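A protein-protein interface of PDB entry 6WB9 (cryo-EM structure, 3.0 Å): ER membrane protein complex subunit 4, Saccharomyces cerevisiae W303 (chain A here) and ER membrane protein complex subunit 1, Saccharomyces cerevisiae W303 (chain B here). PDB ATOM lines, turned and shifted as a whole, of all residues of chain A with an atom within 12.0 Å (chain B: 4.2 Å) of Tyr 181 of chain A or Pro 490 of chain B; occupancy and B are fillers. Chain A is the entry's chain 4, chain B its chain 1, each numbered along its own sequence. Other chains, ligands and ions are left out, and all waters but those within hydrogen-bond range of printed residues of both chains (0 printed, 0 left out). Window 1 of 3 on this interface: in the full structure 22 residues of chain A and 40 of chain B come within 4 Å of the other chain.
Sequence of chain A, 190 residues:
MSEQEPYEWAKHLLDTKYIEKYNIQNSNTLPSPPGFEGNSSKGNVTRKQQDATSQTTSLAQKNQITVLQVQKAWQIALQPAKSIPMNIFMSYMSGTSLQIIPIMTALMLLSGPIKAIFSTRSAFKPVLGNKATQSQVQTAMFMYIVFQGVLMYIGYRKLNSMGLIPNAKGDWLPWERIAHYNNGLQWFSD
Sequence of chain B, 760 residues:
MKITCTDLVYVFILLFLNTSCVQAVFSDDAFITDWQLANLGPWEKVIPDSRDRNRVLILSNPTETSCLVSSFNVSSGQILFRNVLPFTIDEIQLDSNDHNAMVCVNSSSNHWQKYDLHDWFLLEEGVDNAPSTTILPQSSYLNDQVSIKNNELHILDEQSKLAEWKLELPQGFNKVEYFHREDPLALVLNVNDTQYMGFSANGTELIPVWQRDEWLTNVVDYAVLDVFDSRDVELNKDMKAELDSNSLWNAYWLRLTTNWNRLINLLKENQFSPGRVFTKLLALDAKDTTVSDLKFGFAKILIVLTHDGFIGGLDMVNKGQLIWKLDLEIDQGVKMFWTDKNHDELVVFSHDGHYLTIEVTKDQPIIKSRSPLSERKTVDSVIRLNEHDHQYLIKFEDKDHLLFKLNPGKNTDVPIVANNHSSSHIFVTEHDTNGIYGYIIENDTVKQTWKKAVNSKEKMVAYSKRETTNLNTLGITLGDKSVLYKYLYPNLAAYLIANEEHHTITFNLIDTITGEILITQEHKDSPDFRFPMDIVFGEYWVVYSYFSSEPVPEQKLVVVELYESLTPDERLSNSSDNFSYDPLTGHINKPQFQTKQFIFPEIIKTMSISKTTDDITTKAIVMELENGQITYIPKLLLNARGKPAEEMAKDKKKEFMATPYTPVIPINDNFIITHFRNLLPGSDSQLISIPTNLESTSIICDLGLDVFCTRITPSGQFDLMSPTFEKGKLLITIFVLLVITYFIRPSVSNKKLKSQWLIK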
ATOM      1  N   GLU A 176     -19.941  -7.024  15.103  1.00  0.00           N
ATOM      2  CA  GLU A 176     -19.106  -5.839  14.982  1.00  0.00           C
ATOM      3  C   GLU A 176     -18.605  -5.480  16.371  1.00  0.00           C
ATOM      4  O   GLU A 176     -19.397  -5.388  17.313  1.00  0.00           O
ATOM      5  CB  GLU A 176     -19.879  -4.671  14.362  1.00  0.00           C
ATOM      6  CG  GLU A 176     -19.006  -3.509  13.938  1.00  0.00           C
ATOM      7  CD  GLU A 176     -19.673  -2.621  12.910  1.00  0.00           C
ATOM      8  OE1 GLU A 176     -20.702  -3.038  12.341  1.00  0.00           O
ATOM      9  OE2 GLU A 176     -19.167  -1.508  12.666  1.00  0.00           O
ATOM     10  N   ARG A 177     -17.299  -5.279  16.496  1.00  0.00           N
ATOM     11  CA  ARG A 177     -16.671  -5.213  17.803  1.00  0.00           C
ATOM     12  C   ARG A 177     -16.829  -3.827  18.422  1.00  0.00           C
ATOM     13  O   ARG A 177     -17.371  -2.899  17.822  1.00  0.00           O
ATOM     14  CB  ARG A 177     -15.201  -5.615  17.702  1.00  0.00           C
ATOM     15  CG  ARG A 177     -15.001  -7.118  17.591  1.00  0.00           C
ATOM     16  CD  ARG A 177     -13.586  -7.483  17.185  1.00  0.00           C
ATOM     17  NE  ARG A 177     -13.251  -6.987  15.853  1.00  0.00           N
ATOM     18  CZ  ARG A 177     -12.353  -6.039  15.616  1.00  0.00           C
ATOM     19  NH1 ARG A 177     -12.109  -5.647  14.373  1.00  0.00           N
ATOM     20  NH2 ARG A 177     -11.691  -5.489  16.623  1.00  0.00           N
ATOM     21  N   ILE A 178     -16.340  -3.697  19.649  1.00  0.00           N
ATOM     22  CA  ILE A 178     -16.540  -2.517  20.478  1.00  0.00           C
ATOM     23  C   ILE A 178     -15.225  -1.765  20.582  1.00  0.00           C
ATOM     24  O   ILE A 178     -14.157  -2.378  20.693  1.00  0.00           O
ATOM     25  CB  ILE A 178     -17.046  -2.914  21.878  1.00  0.00           C
ATOM     26  CG1 ILE A 178     -18.040  -4.071  21.768  1.00  0.00           C
ATOM     27  CG2 ILE A 178     -17.658  -1.715  22.588  1.00  0.00           C
ATOM     28  CD1 ILE A 178     -18.172  -4.884  23.032  1.00  0.00           C
ATOM     29  N   ALA A 179     -15.301  -0.440  20.540  1.00  0.00           N
ATOM     30  CA  ALA A 179     -14.137   0.378  20.841  1.00  0.00           C
ATOM     31  C   ALA A 179     -13.847   0.296  22.332  1.00  0.00           C
ATOM     32  O   ALA A 179     -14.664   0.718  23.154  1.00  0.00           O
ATOM     33  CB  ALA A 179     -14.375   1.822  20.414  1.00  0.00           C
ATOM     34  N   HIS A 180     -12.697  -0.269  22.685  1.00  0.00           N
ATOM     35  CA  HIS A 180     -12.300  -0.382  24.085  1.00  0.00           C
ATOM     36  C   HIS A 180     -11.694   0.947  24.501  1.00  0.00           C
ATOM     37  O   HIS A 180     -10.541   1.249  24.186  1.00  0.00           O
ATOM     38  CB  HIS A 180     -11.333  -1.543  24.279  1.00  0.00           C
ATOM     39  CG  HIS A 180     -11.942  -2.881  24.000  1.00  0.00           C
ATOM     40  ND1 HIS A 180     -12.867  -3.466  24.839  1.00  0.00           N
ATOM     41  CD2 HIS A 180     -11.765  -3.746  22.974  1.00  0.00           C
ATOM     42  CE1 HIS A 180     -13.232  -4.633  24.341  1.00  0.00           C
ATOM     43  NE2 HIS A 180     -12.579  -4.827  23.211  1.00  0.00           N
ATOM     44  N   TYR A 181     -12.480   1.752  25.216  1.00  0.00           N
ATOM     45  CA  TYR A 181     -12.101   3.137  25.459  1.00  0.00           C
ATOM     46  C   TYR A 181     -11.149   3.282  26.636  1.00  0.00           C
ATOM     47  O   TYR A 181     -10.179   4.041  26.553  1.00  0.00           O
ATOM     48  CB  TYR A 181     -13.345   3.988  25.685  1.00  0.00           C
ATOM     49  CG  TYR A 181     -14.048   4.399  24.417  1.00  0.00           C
ATOM     50  CD1 TYR A 181     -13.545   5.418  23.627  1.00  0.00           C
ATOM     51  CD2 TYR A 181     -15.218   3.773  24.016  1.00  0.00           C
ATOM     52  CE1 TYR A 181     -14.186   5.806  22.477  1.00  0.00           C
ATOM     53  CE2 TYR A 181     -15.865   4.150  22.864  1.00  0.00           C
ATOM     54  CZ  TYR A 181     -15.345   5.168  22.099  1.00  0.00           C
ATOM     55  OH  TYR A 181     -15.988   5.551  20.950  1.00  0.00           O
ATOM     56  N   ASN A 182     -11.402   2.578  27.738  1.00  0.00           N
ATOM     57  CA  ASN A 182     -10.617   2.812  28.949  1.00  0.00           C
ATOM     58  C   ASN A 182      -9.232   2.180  28.839  1.00  0.00           C
ATOM     59  O   ASN A 182      -8.225   2.894  28.780  1.00  0.00           O
ATOM     60  CB  ASN A 182     -11.375   2.283  30.170  1.00  0.00           C
ATOM     61  CG  ASN A 182     -12.659   3.045  30.431  1.00  0.00           C
ATOM     62  OD1 ASN A 182     -12.735   4.251  30.208  1.00  0.00           O
ATOM     63  ND2 ASN A 182     -13.674   2.342  30.908  1.00  0.00           N
ATOM     64  N   ASN A 183      -9.184   0.843  28.772  1.00  0.00           N
ATOM     65  CA  ASN A 183      -7.969   0.048  28.534  1.00  0.00           C
ATOM     66  C   ASN A 183      -6.858   0.360  29.534  1.00  0.00           C
ATOM     67  O   ASN A 183      -5.693   0.541  29.172  1.00  0.00           O
ATOM     68  CB  ASN A 183      -7.466   0.221  27.099  1.00  0.00           C
ATOM     69  CG  ASN A 183      -8.169  -0.694  26.121  1.00  0.00           C
ATOM     70  OD1 ASN A 183      -8.692  -1.742  26.499  1.00  0.00           O
ATOM     71  ND2 ASN A 183      -8.177  -0.307  24.852  1.00  0.00           N
ATOM     72  N   GLY A 184      -7.225   0.435  30.807  1.00  0.00           N
ATOM     73  CA  GLY A 184      -6.229   0.699  31.824  1.00  0.00           C
ATOM     74  C   GLY A 184      -6.562   1.850  32.747  1.00  0.00           C
ATOM     75  O   GLY A 184      -5.674   2.391  33.412  1.00  0.00           O
ATOM     76  N   LEU A 185      -7.832   2.245  32.791  1.00  0.00           N
ATOM     77  CA  LEU A 185      -8.298   3.189  33.793  1.00  0.00           C
ATOM     78  C   LEU A 185      -9.704   2.804  34.224  1.00  0.00           C
ATOM     79  O   LEU A 185     -10.410   2.065  33.535  1.00  0.00           O
ATOM     80  CB  LEU A 185      -8.262   4.640  33.291  1.00  0.00           C
ATOM     81  CG  LEU A 185      -9.066   5.092  32.074  1.00  0.00           C
ATOM     82  CD1 LEU A 185     -10.358   5.778  32.471  1.00  0.00           C
ATOM     83  CD2 LEU A 185      -8.209   6.026  31.253  1.00  0.00           C
ATOM     84  N   GLN A 186     -10.097   3.317  35.384  1.00  0.00           N
ATOM     85  CA  GLN A 186     -11.410   3.074  35.954  1.00  0.00           C
ATOM     86  C   GLN A 186     -12.020   4.401  36.369  1.00  0.00           C
ATOM     87  O   GLN A 186     -11.308   5.340  36.729  1.00  0.00           O
ATOM     88  CB  GLN A 186     -11.338   2.139  37.159  1.00  0.00           C
ATOM     89  CG  GLN A 186     -10.970   0.713  36.823  1.00  0.00           C
ATOM     90  CD  GLN A 186     -10.706  -0.110  38.057  1.00  0.00           C
ATOM     91  OE1 GLN A 186      -9.660   0.025  38.689  1.00  0.00           O
ATOM     92  NE2 GLN A 186     -11.655  -0.962  38.416  1.00  0.00           N
ATOM     93  N   TRP A 187     -13.344   4.471  36.317  1.00  0.00           N
ATOM     94  CA  TRP A 187     -14.054   5.710  36.586  1.00  0.00           C
ATOM     95  C   TRP A 187     -15.235   5.452  37.507  1.00  0.00           C
ATOM     96  O   TRP A 187     -16.059   4.571  37.237  1.00  0.00           O
ATOM     97  CB  TRP A 187     -14.520   6.352  35.288  1.00  0.00           C
ATOM     98  CG  TRP A 187     -15.330   7.556  35.507  1.00  0.00           C
ATOM     99  CD1 TRP A 187     -14.899   8.750  35.979  1.00  0.00           C
ATOM    100  CD2 TRP A 187     -16.728   7.698  35.258  1.00  0.00           C
ATOM    101  NE1 TRP A 187     -15.941   9.631  36.044  1.00  0.00           N
ATOM    102  CE2 TRP A 187     -17.079   9.008  35.609  1.00  0.00           C
ATOM    103  CE3 TRP A 187     -17.719   6.838  34.782  1.00  0.00           C
ATOM    104  CZ2 TRP A 187     -18.374   9.485  35.490  1.00  0.00           C
ATOM    105  CZ3 TRP A 187     -19.001   7.315  34.661  1.00  0.00           C
ATOM    106  CH2 TRP A 187     -19.318   8.624  35.013  1.00  0.00           C
ATOM    107  N   PHE A 188     -15.314   6.223  38.590  1.00  0.00           N
ATOM    108  CA  PHE A 188     -16.359   6.098  39.594  1.00  0.00           C
ATOM    109  C   PHE A 188     -16.904   7.483  39.903  1.00  0.00           C
ATOM    110  O   PHE A 188     -16.174   8.467  39.859  1.00  0.00           O
ATOM    111  CB  PHE A 188     -15.818   5.428  40.860  1.00  0.00           C
ATOM    112  CG  PHE A 188     -15.040   4.180  40.581  1.00  0.00           C
ATOM    113  CD1 PHE A 188     -15.694   2.994  40.308  1.00  0.00           C
ATOM    114  CD2 PHE A 188     -13.659   4.201  40.554  1.00  0.00           C
ATOM    115  CE1 PHE A 188     -14.987   1.851  40.031  1.00  0.00           C
ATOM    116  CE2 PHE A 188     -12.948   3.059  40.275  1.00  0.00           C
ATOM    117  CZ  PHE A 188     -13.612   1.887  40.011  1.00  0.00           C
ATOM    118  N   SER A 189     -18.195   7.571  40.193  1.00  0.00           N
ATOM    119  CA  SER A 189     -18.821   8.875  40.326  1.00  0.00           C
ATOM    120  C   SER A 189     -19.612   8.974  41.621  1.00  0.00           C
ATOM    121  O   SER A 189     -19.941   7.972  42.260  1.00  0.00           O
ATOM    122  CB  SER A 189     -19.734   9.175  39.140  1.00  0.00           C
ATOM    123  OG  SER A 189     -20.242  10.494  39.207  1.00  0.00           O
ATOM    124  N   ARG B 466     -23.018   8.372  33.696  1.00  0.00           N
ATOM    125  CA  ARG B 466     -23.451   7.398  32.707  1.00  0.00           C
ATOM    126  C   ARG B 466     -23.461   6.020  33.347  1.00  0.00           C
ATOM    127  O   ARG B 466     -22.423   5.536  33.809  1.00  0.00           O
ATOM    128  CB  ARG B 466     -22.538   7.416  31.489  1.00  0.00           C
ATOM    129  CG  ARG B 466     -23.073   6.595  30.340  1.00  0.00           C
ATOM    130  CD  ARG B 466     -22.041   6.417  29.259  1.00  0.00           C
ATOM    131  NE  ARG B 466     -22.454   5.423  28.280  1.00  0.00           N
ATOM    132  CZ  ARG B 466     -22.229   4.121  28.403  1.00  0.00           C
ATOM    133  NH1 ARG B 466     -22.639   3.287  27.465  1.00  0.00           N
ATOM    134  NH2 ARG B 466     -21.594   3.655  29.465  1.00  0.00           N
ATOM    135  N   LEU B 488     -21.226   5.077  22.610  1.00  0.00           N
ATOM    136  CA  LEU B 488     -21.030   4.182  23.741  1.00  0.00           C
ATOM    137  C   LEU B 488     -19.730   4.444  24.471  1.00  0.00           C
ATOM    138  O   LEU B 488     -19.188   3.534  25.109  1.00  0.00           O
ATOM    139  CB  LEU B 488     -21.079   2.732  23.274  1.00  0.00           C
ATOM    140  CG  LEU B 488     -22.339   2.364  22.513  1.00  0.00           C
ATOM    141  CD1 LEU B 488     -22.098   1.114  21.724  1.00  0.00           C
ATOM    142  CD2 LEU B 488     -23.481   2.183  23.474  1.00  0.00           C
ATOM    143  N   TYR B 489     -19.208   5.649  24.376  1.00  0.00           N
ATOM    144  CA  TYR B 489     -18.033   6.007  25.138  1.00  0.00           C
ATOM    145  C   TYR B 489     -18.425   6.141  26.600  1.00  0.00           C
ATOM    146  O   TYR B 489     -19.316   6.933  26.921  1.00  0.00           O
ATOM    147  CB  TYR B 489     -17.433   7.302  24.607  1.00  0.00           C
ATOM    148  CG  TYR B 489     -16.457   7.973  25.537  1.00  0.00           C
ATOM    149  CD1 TYR B 489     -15.290   7.339  25.934  1.00  0.00           C
ATOM    150  CD2 TYR B 489     -16.691   9.255  25.996  1.00  0.00           C
ATOM    151  CE1 TYR B 489     -14.397   7.953  26.778  1.00  0.00           C
ATOM    152  CE2 TYR B 489     -15.807   9.876  26.836  1.00  0.00           C
ATOM    153  CZ  TYR B 489     -14.661   9.220  27.227  1.00  0.00           C
ATOM    154  OH  TYR B 489     -13.771   9.842  28.069  1.00  0.00           O
ATOM    155  N   PRO B 490     -17.795   5.401  27.511  1.00  0.00           N
ATOM    156  CA  PRO B 490     -18.095   5.563  28.937  1.00  0.00           C
ATOM    157  C   PRO B 490     -17.487   6.836  29.492  1.00  0.00           C
ATOM    158  O   PRO B 490     -17.017   7.680  28.727  1.00  0.00           O
ATOM    159  CB  PRO B 490     -17.464   4.320  29.564  1.00  0.00           C
ATOM    160  CG  PRO B 490     -16.330   4.015  28.674  1.00  0.00           C
ATOM    161  CD  PRO B 490     -16.781   4.357  27.288  1.00  0.00           C
ATOM    162  N   ASN B 491     -17.512   6.984  30.818  1.00  0.00           N
ATOM    163  CA  ASN B 491     -16.944   8.134  31.531  1.00  0.00           C
ATOM    164  C   ASN B 491     -17.618   9.432  31.106  1.00  0.00           C
ATOM    165  O   ASN B 491     -16.972  10.456  30.934  1.00  0.00           O
ATOM    166  CB  ASN B 491     -15.420   8.239  31.369  1.00  0.00           C
ATOM    167  CG  ASN B 491     -14.740   6.890  31.324  1.00  0.00           C
ATOM    168  OD1 ASN B 491     -15.139   5.958  32.018  1.00  0.00           O
ATOM    169  ND2 ASN B 491     -13.716   6.773  30.494  1.00  0.00           N
ATOM    170  N   LEU B 492     -18.925   9.395  30.931  1.00  0.00           N
ATOM    171  CA  LEU B 492     -19.676  10.596  30.621  1.00  0.00           C
ATOM    172  C   LEU B 492     -20.487  11.004  31.837  1.00  0.00           C
ATOM    173  O   LEU B 492     -20.930  10.156  32.613  1.00  0.00           O
ATOM    174  CB  LEU B 492     -20.601  10.378  29.424  1.00  0.00           C
ATOM    175  CG  LEU B 492     -19.918  10.169  28.079  1.00  0.00           C
ATOM    176  CD1 LEU B 492     -20.944   9.892  27.008  1.00  0.00           C
ATOM    177  CD2 LEU B 492     -19.111  11.390  27.742  1.00  0.00           C
ATOM    178  N   GLU B 564     -22.379   8.527  17.366  1.00  0.00           N
ATOM    179  CA  GLU B 564     -21.032   8.828  16.896  1.00  0.00           C
ATOM    180  C   GLU B 564     -21.062   9.783  15.716  1.00  0.00           C
ATOM    181  O   GLU B 564     -20.166  10.622  15.574  1.00  0.00           O
ATOM    182  CB  GLU B 564     -20.306   7.543  16.526  1.00  0.00           C
ATOM    183  CG  GLU B 564     -19.905   6.730  17.725  1.00  0.00           C
ATOM    184  CD  GLU B 564     -19.421   5.363  17.344  1.00  0.00           C
ATOM    185  OE1 GLU B 564     -19.445   5.056  16.141  1.00  0.00           O
ATOM    186  OE2 GLU B 564     -19.021   4.595  18.243  1.00  0.00           O
ATOM    187  N   SER B 573     -15.667   5.498  15.763  1.00  0.00           N
ATOM    188  CA  SER B 573     -14.838   4.875  16.783  1.00  0.00           C
ATOM    189  C   SER B 573     -13.978   3.789  16.157  1.00  0.00           C
ATOM    190  O   SER B 573     -14.425   3.069  15.260  1.00  0.00           O
ATOM    191  CB  SER B 573     -15.700   4.284  17.897  1.00  0.00           C
ATOM    192  OG  SER B 573     -16.617   3.342  17.379  1.00  0.00           O
ATOM    193  N   TYR B 581      -7.737   3.118  22.843  1.00  0.00           N
ATOM    194  CA  TYR B 581      -8.039   4.505  23.160  1.00  0.00           C
ATOM    195  C   TYR B 581      -7.410   4.903  24.487  1.00  0.00           C
ATOM    196  O   TYR B 581      -7.339   4.108  25.426  1.00  0.00           O
ATOM    197  CB  TYR B 581      -9.549   4.727  23.220  1.00  0.00           C
ATOM    198  CG  TYR B 581     -10.187   5.046  21.894  1.00  0.00           C
ATOM    199  CD1 TYR B 581     -10.051   6.303  21.327  1.00  0.00           C
ATOM    200  CD2 TYR B 581     -10.940   4.098  21.218  1.00  0.00           C
ATOM    201  CE1 TYR B 581     -10.636   6.605  20.119  1.00  0.00           C
ATOM    202  CE2 TYR B 581     -11.531   4.394  20.008  1.00  0.00           C
ATOM    203  CZ  TYR B 581     -11.374   5.650  19.465  1.00  0.00           C
ATOM    204  OH  TYR B 581     -11.957   5.952  18.260  1.00  0.00           O
ATOM    205  N   PRO B 583      -8.282   7.998  26.805  1.00  0.00           N
ATOM    206  CA  PRO B 583      -9.119   9.192  26.971  1.00  0.00           C
ATOM    207  C   PRO B 583      -8.518  10.253  27.871  1.00  0.00           C
ATOM    208  O   PRO B 583      -9.079  11.351  27.952  1.00  0.00           O
ATOM    209  CB  PRO B 583     -10.408   8.624  27.575  1.00  0.00           C
ATOM    210  CG  PRO B 583      -9.972   7.431  28.309  1.00  0.00           C
ATOM    211  CD  PRO B 583      -8.804   6.852  27.566  1.00  0.00           C
ATOM    212  N   ASN B 589     -13.536  10.010  20.111  1.00  0.00           N
ATOM    213  CA  ASN B 589     -14.495  10.574  19.178  1.00  0.00           C
ATOM    214  C   ASN B 589     -15.506  11.439  19.921  1.00  0.00           C
ATOM    215  O   ASN B 589     -15.820  11.204  21.089  1.00  0.00           O
ATOM    216  CB  ASN B 589     -15.207   9.472  18.399  1.00  0.00           C
ATOM    217  CG  ASN B 589     -15.642   8.331  19.277  1.00  0.00           C
ATOM    218  OD1 ASN B 589     -14.872   7.838  20.093  1.00  0.00           O
ATOM    219  ND2 ASN B 589     -16.883   7.901  19.116  1.00  0.00           N
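Of the 11 printed residues of chain B, 9 touch a printed residue of chain A.
Hydrophobic or aromatic side chains of chain A within 4 Å of the printed part of chain B: Ala 179, Tyr 181, Leu 185 and Trp 187.
Among the printed residues, no Asp or Glu carboxylate lies within 4 Å of a Lys or Arg side-chain nitrogen of the other chain.
ND2 of Asn 491 of chain B is in hydrogen-bond range of OD1 of Asn 182 of chain A.
OD1 of Asn 589 of chain B lies within hydrogen-bond range of OH of Tyr 181 of chain A, at 2.7 Å.
The backbone carbonyl oxygen (O) of Tyr 581 of chain B sits close to the backbone carbonyl oxygen (O) of Tyr 181 of chain A.
Glu 176 of chain A touches none of the printed residues of chain B.
Of the printed residues of chain B, Ala 179 of chain A touches Ser 573 and Tyr 581.
Tyr 181 of chain A touches six residues of chain B.
Gln 186 of chain A touches none of the printed residues of chain B.
Of chain A, only Trp 187 comes within 4 Å of Arg 466 of chain B.
No residue of chain A comes within 4 Å of Leu 488 of chain B.
Of chain A, only Tyr 181 comes within 4 Å of Tyr 489 of chain B.
Of chain A, only Tyr 181 and Asn 182 come within 4 Å of Pro 490 of chain B.
Of chain A, only Asn 182 and Trp 187 come within 4 Å of Asn 491 of chain B.
Printed residues of chain A within 4 Å of Tyr 581 of chain B: Ala 179, His 180, Tyr 181, Asn 182 and Asn 183.
Asn 589 of chain B touches one residue of chain A.
The backbone NH (N) of Arg 466 of chain B is in hydrogen-bond range of the backbone carbonyl oxygen (O) of Leu 492 of chain B (3.0 Å).
The side-chain carboxylate (OE2) of Glu 564 of chain B lies within hydrogen-bond range of the side-chain hydroxyl (OG) of Ser 573 of chain B (2.8 Å).
The side-chain amide nitrogen (ND2) of Asn 183 of chain A sits at hydrogen-bond distance from the backbone carbonyl oxygen (O) of His 180 of chain A (2.9 Å).
Among the printed residues, pairs that only touch across the chains: Trp 187 of chain A with Leu 492 of chain B (3.3 Å), Tyr 181 of chain A with Pro 583 of chain B (3.3 Å), Tyr 181 of chain A with Ser 573 of chain B (3.3 Å), Trp 187 of chain A with Asn 491 of chain B (3.4 Å), Tyr 181 of chain A with Tyr 489 of chain B (3.5 Å), His 180 of chain A with Tyr 581 of chain B (3.6 Å), Tyr 181 of chain A with Pro 490 of chain B (3.7 Å), Asn 182 of chain A with Tyr 581 of chain B (3.7 Å), Leu 185 of chain A with Pro 583 of chain B (3.7 Å), Ala 179 of chain A with Ser 573 of chain B (3.8 Å), Asn 182 of chain A with Pro 490 of chain B (3.9 Å), Ala 179 of chain A with Tyr 581 of chain B (3.9 Å), Trp 187 of chain A with Arg 466 of chain B (3.9 Å) and Asn 183 of chain A with Tyr 581 of chain B (3.995 Å).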
